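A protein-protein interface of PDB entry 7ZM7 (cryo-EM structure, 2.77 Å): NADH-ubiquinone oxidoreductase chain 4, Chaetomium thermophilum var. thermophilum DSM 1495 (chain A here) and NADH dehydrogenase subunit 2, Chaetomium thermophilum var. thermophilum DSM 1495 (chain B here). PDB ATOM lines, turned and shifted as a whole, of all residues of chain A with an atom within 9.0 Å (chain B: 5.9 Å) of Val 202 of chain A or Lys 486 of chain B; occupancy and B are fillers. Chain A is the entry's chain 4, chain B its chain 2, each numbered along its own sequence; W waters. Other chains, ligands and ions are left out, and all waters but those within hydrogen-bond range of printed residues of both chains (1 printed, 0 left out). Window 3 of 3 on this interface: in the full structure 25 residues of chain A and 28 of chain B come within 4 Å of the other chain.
The side-chain amino group of Lys 486 of chain B lies close to the backbone carbonyl oxygen of Asn 483 of chain B, at 3.4 Å.
NZ of Lys 486 of chain B lies within salt-bridge range of OE1 of Glu 487 of chain B.
NZ of Lys 201 of chain A is in hydrogen-bond range of O of Gly 194 of chain A, 2.8 Å away.
The backbone carbonyl oxygen (O) of Lys 201 of chain A lies within hydrogen-bond range of the side-chain hydroxyl (OG) of Ser 205 of chain A, at 3.3 Å.
O of Val 202 of chain A sits at hydrogen-bond distance from OG of Ser 205 of chain A (2.8 Å).
Of the printed residues of chain B, Phe 190 of chain A touches Leu 482, Ile 485 and Phe 490.
Of chain B, only Lys 486 and Phe 490 come within 4 Å of Val 202 of chain A.
Of the printed residues of chain B, Ser 205 of chain A touches Phe 490.
Of the printed residues of chain B, Phe 206 of chain A touches Leu 482 and Asn 483.
Printed residues of chain B within 4 Å of Leu 210 of chain A: Leu 482 (3.99 Å).
Lys 486 of chain B touches just one residue of chain A: Val 202 (3.9 Å).
The nearest residue of chain A that does not touch Lys 486 of chain B is Phe 206 of chain A (4.1 Å).
The nearest printed residue of chain A that does not touch Asn 483 of chain B is Phe 190 of chain A (5.6 Å).
Among the printed residues, pairs that only touch across the chains: Phe 190 of chain A with Phe 490 of chain B, Leu 195 of chain A with Phe 489 of chain B, Ser 205 of chain A with Phe 490 of chain B, Phe 206 of chain A with Asn 483 of chain B, Phe 206 of chain A with Leu 482 of chain B, Gly 194 of chain A with Phe 490 of chain B, Ile 191 of chain A with Phe 490 of chain B, Phe 209 of chain A with Leu 482 of chain B, Phe 190 of chain A with Leu 482 of chain B, Phe 190 of chain A with Ile 485 of chain B, Ile 191 of chain A with Ile 485 of chain B, Val 202 of chain A with Lys 486 of chain B, Val 202 of chain A with Phe 490 of chain B, Ile 191 of chain A with Phe 489 of chain B and Leu 210 of chain A with Leu 482 of chain B.
Water W1 bridges the side-chain amino group of Lys 201 of chain A and the backbone carbonyl oxygen of Phe 490 of chain B.
Of the 11 printed residues of chain B, 6 touch a printed residue of chain A.
Hydrophobic or aromatic side chains of chain B within 4 Å of the printed part of chain A: Leu 482, Ile 485, Phe 489 and Phe 490.
Hydrophobic or aromatic side chains of chain A that line the printed part of chain B: Phe 190, Ile 191, Leu 195, Val 202, Phe 206, Phe 209 and Leu 210.
Among the printed residues, 15 pairs touch across the chains.
Among the printed residues, no Asp or Glu carboxylate lies within 4 Å of a Lys or Arg side-chain nitrogen of the other chain.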
ATOM      1  N   LEU A 189      23.791  -1.001 -10.856  1.00  0.00           N
ATOM      2  CA  LEU A 189      22.531  -1.702 -10.662  1.00  0.00           C
ATOM      3  C   LEU A 189      22.324  -2.783 -11.705  1.00  0.00           C
ATOM      4  O   LEU A 189      21.623  -3.759 -11.447  1.00  0.00           O
ATOM      5  CB  LEU A 189      21.372  -0.716 -10.690  1.00  0.00           C
ATOM      6  CG  LEU A 189      21.062   0.003  -9.386  1.00  0.00           C
ATOM      7  CD1 LEU A 189      20.272   1.255  -9.662  1.00  0.00           C
ATOM      8  CD2 LEU A 189      20.300  -0.911  -8.463  1.00  0.00           C
ATOM      9  N   PHE A 190      22.910  -2.615 -12.886  1.00  0.00           N
ATOM     10  CA  PHE A 190      22.926  -3.679 -13.882  1.00  0.00           C
ATOM     11  C   PHE A 190      23.713  -4.878 -13.377  1.00  0.00           C
ATOM     12  O   PHE A 190      23.367  -6.021 -13.680  1.00  0.00           O
ATOM     13  CB  PHE A 190      23.505  -3.130 -15.186  1.00  0.00           C
ATOM     14  CG  PHE A 190      23.546  -4.112 -16.306  1.00  0.00           C
ATOM     15  CD1 PHE A 190      22.393  -4.487 -16.952  1.00  0.00           C
ATOM     16  CD2 PHE A 190      24.745  -4.637 -16.732  1.00  0.00           C
ATOM     17  CE1 PHE A 190      22.427  -5.375 -17.971  1.00  0.00           C
ATOM     18  CE2 PHE A 190      24.787  -5.533 -17.760  1.00  0.00           C
ATOM     19  CZ  PHE A 190      23.630  -5.896 -18.380  1.00  0.00           C
ATOM     20  N   ILE A 191      24.755  -4.631 -12.588  1.00  0.00           N
ATOM     21  CA  ILE A 191      25.596  -5.692 -12.060  1.00  0.00           C
ATOM     22  C   ILE A 191      25.077  -6.205 -10.726  1.00  0.00           C
ATOM     23  O   ILE A 191      25.246  -7.384 -10.401  1.00  0.00           O
ATOM     24  CB  ILE A 191      27.038  -5.183 -11.968  1.00  0.00           C
ATOM     25  CG1 ILE A 191      27.554  -4.882 -13.365  1.00  0.00           C
ATOM     26  CG2 ILE A 191      27.941  -6.173 -11.273  1.00  0.00           C
ATOM     27  CD1 ILE A 191      27.632  -6.076 -14.231  1.00  0.00           C
ATOM     28  N   ILE A 193      22.076  -6.789 -10.176  1.00  0.00           N
ATOM     29  CA  ILE A 193      20.937  -7.697 -10.487  1.00  0.00           C
ATOM     30  C   ILE A 193      21.467  -8.946 -11.199  1.00  0.00           C
ATOM     31  O   ILE A 193      21.034 -10.037 -10.851  1.00  0.00           O
ATOM     32  CB  ILE A 193      19.797  -6.976 -11.248  1.00  0.00           C
ATOM     33  CG1 ILE A 193      19.339  -5.706 -10.536  1.00  0.00           C
ATOM     34  CG2 ILE A 193      18.631  -7.913 -11.510  1.00  0.00           C
ATOM     35  CD1 ILE A 193      18.189  -5.001 -11.209  1.00  0.00           C
ATOM     36  N   GLY A 194      22.390  -8.799 -12.134  1.00  0.00           N
ATOM     37  CA  GLY A 194      22.894  -9.953 -12.894  1.00  0.00           C
ATOM     38  C   GLY A 194      23.844 -10.812 -12.093  1.00  0.00           C
ATOM     39  O   GLY A 194      23.885 -12.009 -12.358  1.00  0.00           O
ATOM     40  N   LEU A 195      24.515 -10.267 -11.077  1.00  0.00           N
ATOM     41  CA  LEU A 195      25.369 -11.136 -10.224  1.00  0.00           C
ATOM     42  C   LEU A 195      24.590 -11.737  -9.059  1.00  0.00           C
ATOM     43  O   LEU A 195      24.813 -12.919  -8.771  1.00  0.00           O
ATOM     44  CB  LEU A 195      26.574 -10.345  -9.716  1.00  0.00           C
ATOM     45  CG  LEU A 195      27.829 -10.384 -10.582  1.00  0.00           C
ATOM     46  CD1 LEU A 195      28.919  -9.520  -9.968  1.00  0.00           C
ATOM     47  CD2 LEU A 195      28.326 -11.808 -10.747  1.00  0.00           C
ATOM     48  N   GLY A 197      21.060 -11.573  -8.552  1.00  0.00           N
ATOM     49  CA  GLY A 197      19.615 -11.672  -8.816  1.00  0.00           C
ATOM     50  C   GLY A 197      19.072 -13.080  -8.950  1.00  0.00           C
ATOM     51  O   GLY A 197      19.872 -14.024  -9.012  1.00  0.00           O
ATOM     52  N   SER A 198      17.751 -13.209  -9.064  1.00  0.00           N
ATOM     53  CA  SER A 198      17.066 -14.528  -9.119  1.00  0.00           C
ATOM     54  C   SER A 198      17.046 -15.101 -10.541  1.00  0.00           C
ATOM     55  O   SER A 198      17.933 -14.762 -11.312  1.00  0.00           O
ATOM     56  CB  SER A 198      15.698 -14.396  -8.540  1.00  0.00           C
ATOM     57  OG  SER A 198      15.736 -13.667  -7.325  1.00  0.00           O
ATOM     58  N   SER A 199      16.127 -16.014 -10.844  1.00  0.00           N
ATOM     59  CA  SER A 199      16.123 -16.715 -12.157  1.00  0.00           C
ATOM     60  C   SER A 199      16.008 -15.780 -13.362  1.00  0.00           C
ATOM     61  O   SER A 199      16.795 -15.959 -14.302  1.00  0.00           O
ATOM     62  CB  SER A 199      15.060 -17.770 -12.187  1.00  0.00           C
ATOM     63  OG  SER A 199      15.074 -18.466 -13.423  1.00  0.00           O
ATOM     64  N   ASN A 200      15.065 -14.843 -13.350  1.00  0.00           N
ATOM     65  CA  ASN A 200      14.833 -13.994 -14.542  1.00  0.00           C
ATOM     66  C   ASN A 200      15.692 -12.733 -14.435  1.00  0.00           C
ATOM     67  O   ASN A 200      15.297 -11.707 -14.998  1.00  0.00           O
ATOM     68  CB  ASN A 200      13.341 -13.749 -14.739  1.00  0.00           C
ATOM     69  CG  ASN A 200      12.546 -15.021 -14.933  1.00  0.00           C
ATOM     70  OD1 ASN A 200      13.086 -16.035 -15.370  1.00  0.00           O
ATOM     71  ND2 ASN A 200      11.262 -14.972 -14.622  1.00  0.00           N
ATOM     72  N   LYS A 201      16.838 -12.829 -13.768  1.00  0.00           N
ATOM     73  CA  LYS A 201      17.741 -11.671 -13.545  1.00  0.00           C
ATOM     74  C   LYS A 201      18.252 -11.032 -14.840  1.00  0.00           C
ATOM     75  O   LYS A 201      18.360  -9.807 -14.860  1.00  0.00           O
ATOM     76  CB  LYS A 201      18.928 -12.130 -12.691  1.00  0.00           C
ATOM     77  CG  LYS A 201      19.856 -13.167 -13.303  1.00  0.00           C
ATOM     78  CD  LYS A 201      20.958 -13.553 -12.354  1.00  0.00           C
ATOM     79  CE  LYS A 201      21.990 -14.469 -12.967  1.00  0.00           C
ATOM     80  NZ  LYS A 201      23.128 -14.685 -12.043  1.00  0.00           N
ATOM     81  N   VAL A 202      18.552 -11.801 -15.889  1.00  0.00           N
ATOM     82  CA  VAL A 202      19.190 -11.179 -17.088  1.00  0.00           C
ATOM     83  C   VAL A 202      18.231 -10.198 -17.768  1.00  0.00           C
ATOM     84  O   VAL A 202      18.633  -9.043 -17.945  1.00  0.00           O
ATOM     85  CB  VAL A 202      19.846 -12.195 -18.046  1.00  0.00           C
ATOM     86  CG1 VAL A 202      20.595 -11.487 -19.160  1.00  0.00           C
ATOM     87  CG2 VAL A 202      20.799 -13.113 -17.301  1.00  0.00           C
ATOM     88  N   ARG A 203      17.007 -10.617 -18.082  1.00  0.00           N
ATOM     89  CA  ARG A 203      16.000  -9.734 -18.724  1.00  0.00           C
ATOM     90  C   ARG A 203      15.672  -8.577 -17.779  1.00  0.00           C
ATOM     91  O   ARG A 203      15.518  -7.455 -18.263  1.00  0.00           O
ATOM     92  CB  ARG A 203      14.757 -10.540 -19.117  1.00  0.00           C
ATOM     93  CG  ARG A 203      13.840  -9.836 -20.104  1.00  0.00           C
ATOM     94  CD  ARG A 203      12.668 -10.673 -20.577  1.00  0.00           C
ATOM     95  NE  ARG A 203      11.858  -9.917 -21.522  1.00  0.00           N
ATOM     96  CZ  ARG A 203      12.012  -9.935 -22.838  1.00  0.00           C
ATOM     97  NH1 ARG A 203      11.231  -9.196 -23.605  1.00  0.00           N
ATOM     98  NH2 ARG A 203      12.940 -10.693 -23.389  1.00  0.00           N
ATOM     99  N   ALA A 204      15.577  -8.847 -16.482  1.00  0.00           N
ATOM    100  CA  ALA A 204      15.223  -7.801 -15.505  1.00  0.00           C
ATOM    101  C   ALA A 204      16.286  -6.701 -15.503  1.00  0.00           C
ATOM    102  O   ALA A 204      15.907  -5.525 -15.391  1.00  0.00           O
ATOM    103  CB  ALA A 204      15.039  -8.407 -14.142  1.00  0.00           C
ATOM    104  N   SER A 205      17.561  -7.072 -15.607  1.00  0.00           N
ATOM    105  CA  SER A 205      18.661  -6.079 -15.557  1.00  0.00           C
ATOM    106  C   SER A 205      18.692  -5.288 -16.865  1.00  0.00           C
ATOM    107  O   SER A 205      19.013  -4.092 -16.822  1.00  0.00           O
ATOM    108  CB  SER A 205      19.978  -6.712 -15.230  1.00  0.00           C
ATOM    109  OG  SER A 205      20.361  -7.635 -16.233  1.00  0.00           O
ATOM    110  N   PHE A 206      18.339  -5.922 -17.979  1.00  0.00           N
ATOM    111  CA  PHE A 206      18.251  -5.175 -19.226  1.00  0.00           C
ATOM    112  C   PHE A 206      17.095  -4.188 -19.180  1.00  0.00           C
ATOM    113  O   PHE A 206      17.186  -3.093 -19.739  1.00  0.00           O
ATOM    114  CB  PHE A 206      18.098  -6.131 -20.409  1.00  0.00           C
ATOM    115  CG  PHE A 206      19.398  -6.643 -20.938  1.00  0.00           C
ATOM    116  CD1 PHE A 206      20.007  -7.734 -20.363  1.00  0.00           C
ATOM    117  CD2 PHE A 206      20.018  -6.033 -22.002  1.00  0.00           C
ATOM    118  CE1 PHE A 206      21.192  -8.201 -20.831  1.00  0.00           C
ATOM    119  CE2 PHE A 206      21.212  -6.510 -22.471  1.00  0.00           C
ATOM    120  CZ  PHE A 206      21.797  -7.586 -21.877  1.00  0.00           C
ATOM    121  N   TYR A 207      15.981  -4.598 -18.579  1.00  0.00           N
ATOM    122  CA  TYR A 207      14.772  -3.739 -18.569  1.00  0.00           C
ATOM    123  C   TYR A 207      15.059  -2.450 -17.800  1.00  0.00           C
ATOM    124  O   TYR A 207      14.849  -1.375 -18.371  1.00  0.00           O
ATOM    125  CB  TYR A 207      13.569  -4.501 -18.010  1.00  0.00           C
ATOM    126  CG  TYR A 207      12.667  -5.132 -19.039  1.00  0.00           C
ATOM    127  CD1 TYR A 207      13.139  -6.106 -19.902  1.00  0.00           C
ATOM    128  CD2 TYR A 207      11.334  -4.777 -19.136  1.00  0.00           C
ATOM    129  CE1 TYR A 207      12.318  -6.698 -20.844  1.00  0.00           C
ATOM    130  CE2 TYR A 207      10.495  -5.362 -20.069  1.00  0.00           C
ATOM    131  CZ  TYR A 207      10.989  -6.328 -20.927  1.00  0.00           C
ATOM    132  OH  TYR A 207      10.177  -6.915 -21.853  1.00  0.00           O
ATOM    133  N   ILE A 208      15.452  -2.503 -16.574  1.00  0.00           N
ATOM    134  CA  ILE A 208      15.689  -1.275 -15.764  1.00  0.00           C
ATOM    135  C   ILE A 208      16.751  -0.423 -16.459  1.00  0.00           C
ATOM    136  O   ILE A 208      16.510   0.765 -16.616  1.00  0.00           O
ATOM    137  CB  ILE A 208      16.071  -1.612 -14.307  1.00  0.00           C
ATOM    138  CG1 ILE A 208      16.359  -0.351 -13.490  1.00  0.00           C
ATOM    139  CG2 ILE A 208      17.220  -2.605 -14.235  1.00  0.00           C
ATOM    140  CD1 ILE A 208      17.120  -0.614 -12.214  1.00  0.00           C
ATOM    141  N   PHE A 209      17.888  -1.060 -16.888  1.00  0.00           N
ATOM    142  CA  PHE A 209      18.955  -0.225 -17.480  1.00  0.00           C
ATOM    143  C   PHE A 209      18.389   0.483 -18.707  1.00  0.00           C
ATOM    144  O   PHE A 209      18.433   1.714 -18.730  1.00  0.00           O
ATOM    145  CB  PHE A 209      20.184  -1.051 -17.875  1.00  0.00           C
ATOM    146  CG  PHE A 209      21.400  -0.236 -18.243  1.00  0.00           C
ATOM    147  CD1 PHE A 209      21.489   0.404 -19.469  1.00  0.00           C
ATOM    148  CD2 PHE A 209      22.460  -0.113 -17.361  1.00  0.00           C
ATOM    149  CE1 PHE A 209      22.604   1.157 -19.801  1.00  0.00           C
ATOM    150  CE2 PHE A 209      23.576   0.640 -17.694  1.00  0.00           C
ATOM    151  CZ  PHE A 209      23.645   1.273 -18.913  1.00  0.00           C
ATOM    152  N   LEU A 210      17.854  -0.250 -19.683  1.00  0.00           N
ATOM    153  CA  LEU A 210      17.440   0.382 -20.969  1.00  0.00           C
ATOM    154  C   LEU A 210      16.270   1.358 -20.814  1.00  0.00           C
ATOM    155  O   LEU A 210      16.319   2.405 -21.471  1.00  0.00           O
ATOM    156  CB  LEU A 210      17.169  -0.707 -22.012  1.00  0.00           C
ATOM    157  CG  LEU A 210      18.398  -1.507 -22.435  1.00  0.00           C
ATOM    158  CD1 LEU A 210      17.998  -2.757 -23.199  1.00  0.00           C
ATOM    159  CD2 LEU A 210      19.351  -0.650 -23.254  1.00  0.00           C
ATOM    160  N   ARG A 274       9.900  -6.253 -13.007  1.00  0.00           N
ATOM    161  CA  ARG A 274      11.003  -7.175 -13.192  1.00  0.00           C
ATOM    162  C   ARG A 274      12.167  -6.863 -12.269  1.00  0.00           C
ATOM    163  O   ARG A 274      12.637  -7.742 -11.553  1.00  0.00           O
ATOM    164  CB  ARG A 274      11.458  -7.129 -14.648  1.00  0.00           C
ATOM    165  CG  ARG A 274      10.571  -7.888 -15.587  1.00  0.00           C
ATOM    166  CD  ARG A 274      11.203  -7.999 -16.956  1.00  0.00           C
ATOM    167  NE  ARG A 274      10.208  -8.262 -17.997  1.00  0.00           N
ATOM    168  CZ  ARG A 274       9.666  -9.450 -18.245  1.00  0.00           C
ATOM    169  NH1 ARG A 274       8.778  -9.582 -19.214  1.00  0.00           N
ATOM    170  NH2 ARG A 274      10.010 -10.504 -17.530  1.00  0.00           N
ATOM    171  N   ALA A 275      12.626  -5.614 -12.269  1.00  0.00           N
ATOM    172  CA  ALA A 275      13.827  -5.238 -11.530  1.00  0.00           C
ATOM    173  C   ALA A 275      13.612  -5.303 -10.024  1.00  0.00           C
ATOM    174  O   ALA A 275      14.476  -5.786  -9.291  1.00  0.00           O
ATOM    175  CB  ALA A 275      14.270  -3.834 -11.941  1.00  0.00           C
ATOM    176  N   GLU A 278      13.411  -9.504  -9.395  1.00  0.00           N
ATOM    177  CA  GLU A 278      14.541 -10.429  -9.661  1.00  0.00           C
ATOM    178  C   GLU A 278      15.774  -9.996  -8.876  1.00  0.00           C
ATOM    179  O   GLU A 278      16.653 -10.817  -8.647  1.00  0.00           O
ATOM    180  CB  GLU A 278      14.762 -10.645 -11.155  1.00  0.00           C
ATOM    181  CG  GLU A 278      13.548 -11.241 -11.839  1.00  0.00           C
ATOM    182  CD  GLU A 278      12.972 -12.490 -11.196  1.00  0.00           C
ATOM    183  OE1 GLU A 278      13.719 -13.472 -11.037  1.00  0.00           O
ATOM    184  OE2 GLU A 278      11.776 -12.476 -10.851  1.00  0.00           O
ATOM    185  N   SER A 279      15.809  -8.747  -8.457  1.00  0.00           N
ATOM    186  CA  SER A 279      16.980  -8.220  -7.732  1.00  0.00           C
ATOM    187  C   SER A 279      17.190  -8.909  -6.387  1.00  0.00           C
ATOM    188  O   SER A 279      16.233  -9.493  -5.880  1.00  0.00           O
ATOM    189  CB  SER A 279      16.837  -6.765  -7.515  1.00  0.00           C
ATOM    190  OG  SER A 279      15.614  -6.479  -6.871  1.00  0.00           O
ATOM    191  N   TYR B 481      26.124  -3.401 -26.241  1.00  0.00           N
ATOM    192  CA  TYR B 481      27.191  -3.169 -25.278  1.00  0.00           C
ATOM    193  C   TYR B 481      26.930  -3.919 -23.984  1.00  0.00           C
ATOM    194  O   TYR B 481      27.865  -4.409 -23.347  1.00  0.00           O
ATOM    195  CB  TYR B 481      27.334  -1.682 -24.995  1.00  0.00           C
ATOM    196  CG  TYR B 481      27.959  -0.872 -26.098  1.00  0.00           C
ATOM    197  CD1 TYR B 481      29.175  -1.226 -26.660  1.00  0.00           C
ATOM    198  CD2 TYR B 481      27.323   0.261 -26.571  1.00  0.00           C
ATOM    199  CE1 TYR B 481      29.728  -0.478 -27.653  1.00  0.00           C
ATOM    200  CE2 TYR B 481      27.863   1.016 -27.566  1.00  0.00           C
ATOM    201  CZ  TYR B 481      29.062   0.654 -28.103  1.00  0.00           C
ATOM    202  OH  TYR B 481      29.581   1.436 -29.096  1.00  0.00           O
ATOM    203  N   LEU B 482      25.663  -3.994 -23.571  1.00  0.00           N
ATOM    204  CA  LEU B 482      25.308  -4.699 -22.351  1.00  0.00           C
ATOM    205  C   LEU B 482      25.441  -6.200 -22.521  1.00  0.00           C
ATOM    206  O   LEU B 482      25.756  -6.906 -21.563  1.00  0.00           O
ATOM    207  CB  LEU B 482      23.886  -4.341 -21.928  1.00  0.00           C
ATOM    208  CG  LEU B 482      23.555  -2.946 -21.391  1.00  0.00           C
ATOM    209  CD1 LEU B 482      22.056  -2.792 -21.250  1.00  0.00           C
ATOM    210  CD2 LEU B 482      24.257  -2.656 -20.090  1.00  0.00           C
ATOM    211  N   ASN B 483      25.217  -6.702 -23.729  1.00  0.00           N
ATOM    212  CA  ASN B 483      25.423  -8.119 -23.991  1.00  0.00           C
ATOM    213  C   ASN B 483      26.869  -8.521 -23.737  1.00  0.00           C
ATOM    214  O   ASN B 483      27.136  -9.620 -23.250  1.00  0.00           O
ATOM    215  CB  ASN B 483      25.020  -8.442 -25.426  1.00  0.00           C
ATOM    216  CG  ASN B 483      23.537  -8.494 -25.611  1.00  0.00           C
ATOM    217  OD1 ASN B 483      23.004  -7.934 -26.556  1.00  0.00           O
ATOM    218  ND2 ASN B 483      22.853  -9.177 -24.713  1.00  0.00           N
ATOM    219  N   VAL B 484      27.818  -7.658 -24.080  1.00  0.00           N
ATOM    220  CA  VAL B 484      29.205  -7.928 -23.727  1.00  0.00           C
ATOM    221  C   VAL B 484      29.392  -7.928 -22.212  1.00  0.00           C
ATOM    222  O   VAL B 484      30.072  -8.796 -21.666  1.00  0.00           O
ATOM    223  CB  VAL B 484      30.142  -6.928 -24.422  1.00  0.00           C
ATOM    224  CG1 VAL B 484      31.531  -7.115 -23.925  1.00  0.00           C
ATOM    225  CG2 VAL B 484      30.106  -7.139 -25.902  1.00  0.00           C
ATOM    226  N   ILE B 485      28.776  -6.974 -21.520  1.00  0.00           N
ATOM    227  CA  ILE B 485      28.969  -6.874 -20.045  1.00  0.00           C
ATOM    228  C   ILE B 485      28.313  -8.091 -19.387  1.00  0.00           C
ATOM    229  O   ILE B 485      28.945  -8.699 -18.504  1.00  0.00           O
ATOM    230  CB  ILE B 485      28.434  -5.536 -19.491  1.00  0.00           C
ATOM    231  CG1 ILE B 485      29.157  -4.343 -20.117  1.00  0.00           C
ATOM    232  CG2 ILE B 485      28.522  -5.499 -17.974  1.00  0.00           C
ATOM    233  CD1 ILE B 485      30.660  -4.423 -20.002  1.00  0.00           C
ATOM    234  N   LYS B 486      27.107  -8.452 -19.826  1.00  0.00           N
ATOM    235  CA  LYS B 486      26.376  -9.592 -19.224  1.00  0.00           C
ATOM    236  C   LYS B 486      27.199 -10.858 -19.447  1.00  0.00           C
ATOM    237  O   LYS B 486      27.212 -11.725 -18.578  1.00  0.00           O
ATOM    238  CB  LYS B 486      24.940  -9.684 -19.752  1.00  0.00           C
ATOM    239  CG  LYS B 486      24.759 -10.296 -21.132  1.00  0.00           C
ATOM    240  CD  LYS B 486      23.967 -11.578 -21.116  1.00  0.00           C
ATOM    241  CE  LYS B 486      23.865 -12.213 -22.485  1.00  0.00           C
ATOM    242  NZ  LYS B 486      25.200 -12.408 -23.094  1.00  0.00           N
ATOM    243  N   GLU B 487      27.840 -10.959 -20.601  1.00  0.00           N
ATOM    244  CA  GLU B 487      28.616 -12.177 -20.907  1.00  0.00           C
ATOM    245  C   GLU B 487      29.844 -12.268 -20.005  1.00  0.00           C
ATOM    246  O   GLU B 487      30.149 -13.368 -19.616  1.00  0.00           O
ATOM    247  CB  GLU B 487      29.010 -12.212 -22.382  1.00  0.00           C
ATOM    248  CG  GLU B 487      29.520 -13.565 -22.843  1.00  0.00           C
ATOM    249  CD  GLU B 487      28.478 -14.667 -22.947  1.00  0.00           C
ATOM    250  OE1 GLU B 487      27.281 -14.380 -22.754  1.00  0.00           O
ATOM    251  OE2 GLU B 487      28.866 -15.813 -23.239  1.00  0.00           O
ATOM    252  N   ILE B 488      30.468 -11.155 -19.614  1.00  0.00           N
ATOM    253  CA  ILE B 488      31.757 -11.257 -18.878  1.00  0.00           C
ATOM    254  C   ILE B 488      31.412 -11.526 -17.415  1.00  0.00           C
ATOM    255  O   ILE B 488      32.130 -12.314 -16.790  1.00  0.00           O
ATOM    256  CB  ILE B 488      32.555  -9.944 -18.999  1.00  0.00           C
ATOM    257  CG1 ILE B 488      32.988  -9.656 -20.436  1.00  0.00           C
ATOM    258  CG2 ILE B 488      33.737  -9.914 -18.044  1.00  0.00           C
ATOM    259  CD1 ILE B 488      33.249  -8.198 -20.682  1.00  0.00           C
ATOM    260  N   PHE B 489      30.345 -10.906 -16.893  1.00  0.00           N
ATOM    261  CA  PHE B 489      30.008 -10.978 -15.441  1.00  0.00           C
ATOM    262  C   PHE B 489      28.839 -11.897 -15.044  1.00  0.00           C
ATOM    263  O   PHE B 489      28.915 -12.449 -13.953  1.00  0.00           O
ATOM    264  CB  PHE B 489      29.636  -9.579 -14.935  1.00  0.00           C
ATOM    265  CG  PHE B 489      30.689  -8.503 -14.960  1.00  0.00           C
ATOM    266  CD1 PHE B 489      30.978  -7.814 -16.127  1.00  0.00           C
ATOM    267  CD2 PHE B 489      31.341  -8.123 -13.800  1.00  0.00           C
ATOM    268  CE1 PHE B 489      31.935  -6.814 -16.146  1.00  0.00           C
ATOM    269  CE2 PHE B 489      32.296  -7.120 -13.820  1.00  0.00           C
ATOM    270  CZ  PHE B 489      32.590  -6.466 -14.991  1.00  0.00           C
ATOM    271  N   PHE B 490      27.820 -12.092 -15.872  1.00  0.00           N
ATOM    272  CA  PHE B 490      26.583 -12.811 -15.435  1.00  0.00           C
ATOM    273  C   PHE B 490      26.734 -14.328 -15.456  1.00  0.00           C
ATOM    274  O   PHE B 490      25.828 -15.013 -14.990  1.00  0.00           O
ATOM    275  CB  PHE B 490      25.365 -12.387 -16.264  1.00  0.00           C
ATOM    276  CG  PHE B 490      24.920 -10.953 -16.118  1.00  0.00           C
ATOM    277  CD1 PHE B 490      25.744  -9.994 -15.554  1.00  0.00           C
ATOM    278  CD2 PHE B 490      23.673 -10.559 -16.567  1.00  0.00           C
ATOM    279  CE1 PHE B 490      25.334  -8.678 -15.440  1.00  0.00           C
ATOM    280  CE2 PHE B 490      23.263  -9.241 -16.459  1.00  0.00           C
ATOM    281  CZ  PHE B 490      24.093  -8.306 -15.890  1.00  0.00           C
ATOM    282  N   TYR B 491      27.842 -14.823 -16.001  1.00  0.00           N
ATOM    283  CA  TYR B 491      28.048 -16.278 -16.149  1.00  0.00           C
ATOM    284  C   TYR B 491      29.384 -16.752 -15.599  1.00  0.00           C
ATOM    285  O   TYR B 491      30.213 -15.909 -15.252  1.00  0.00           O
ATOM    286  CB  TYR B 491      27.928 -16.663 -17.618  1.00  0.00           C
ATOM    287  CG  TYR B 491      26.683 -16.155 -18.286  1.00  0.00           C
ATOM    288  CD1 TYR B 491      25.438 -16.656 -17.950  1.00  0.00           C
ATOM    289  CD2 TYR B 491      26.754 -15.165 -19.247  1.00  0.00           C
ATOM    290  CE1 TYR B 491      24.287 -16.181 -18.552  1.00  0.00           C
ATOM    291  CE2 TYR B 491      25.614 -14.686 -19.863  1.00  0.00           C
ATOM    292  CZ  TYR B 491      24.380 -15.194 -19.514  1.00  0.00           C
ATOM    293  OH  TYR B 491      23.263 -14.713 -20.121  1.00  0.00           O
HETATM  294  O   HOH W   1      26.337 -14.533 -11.589  1.00  0.00           O
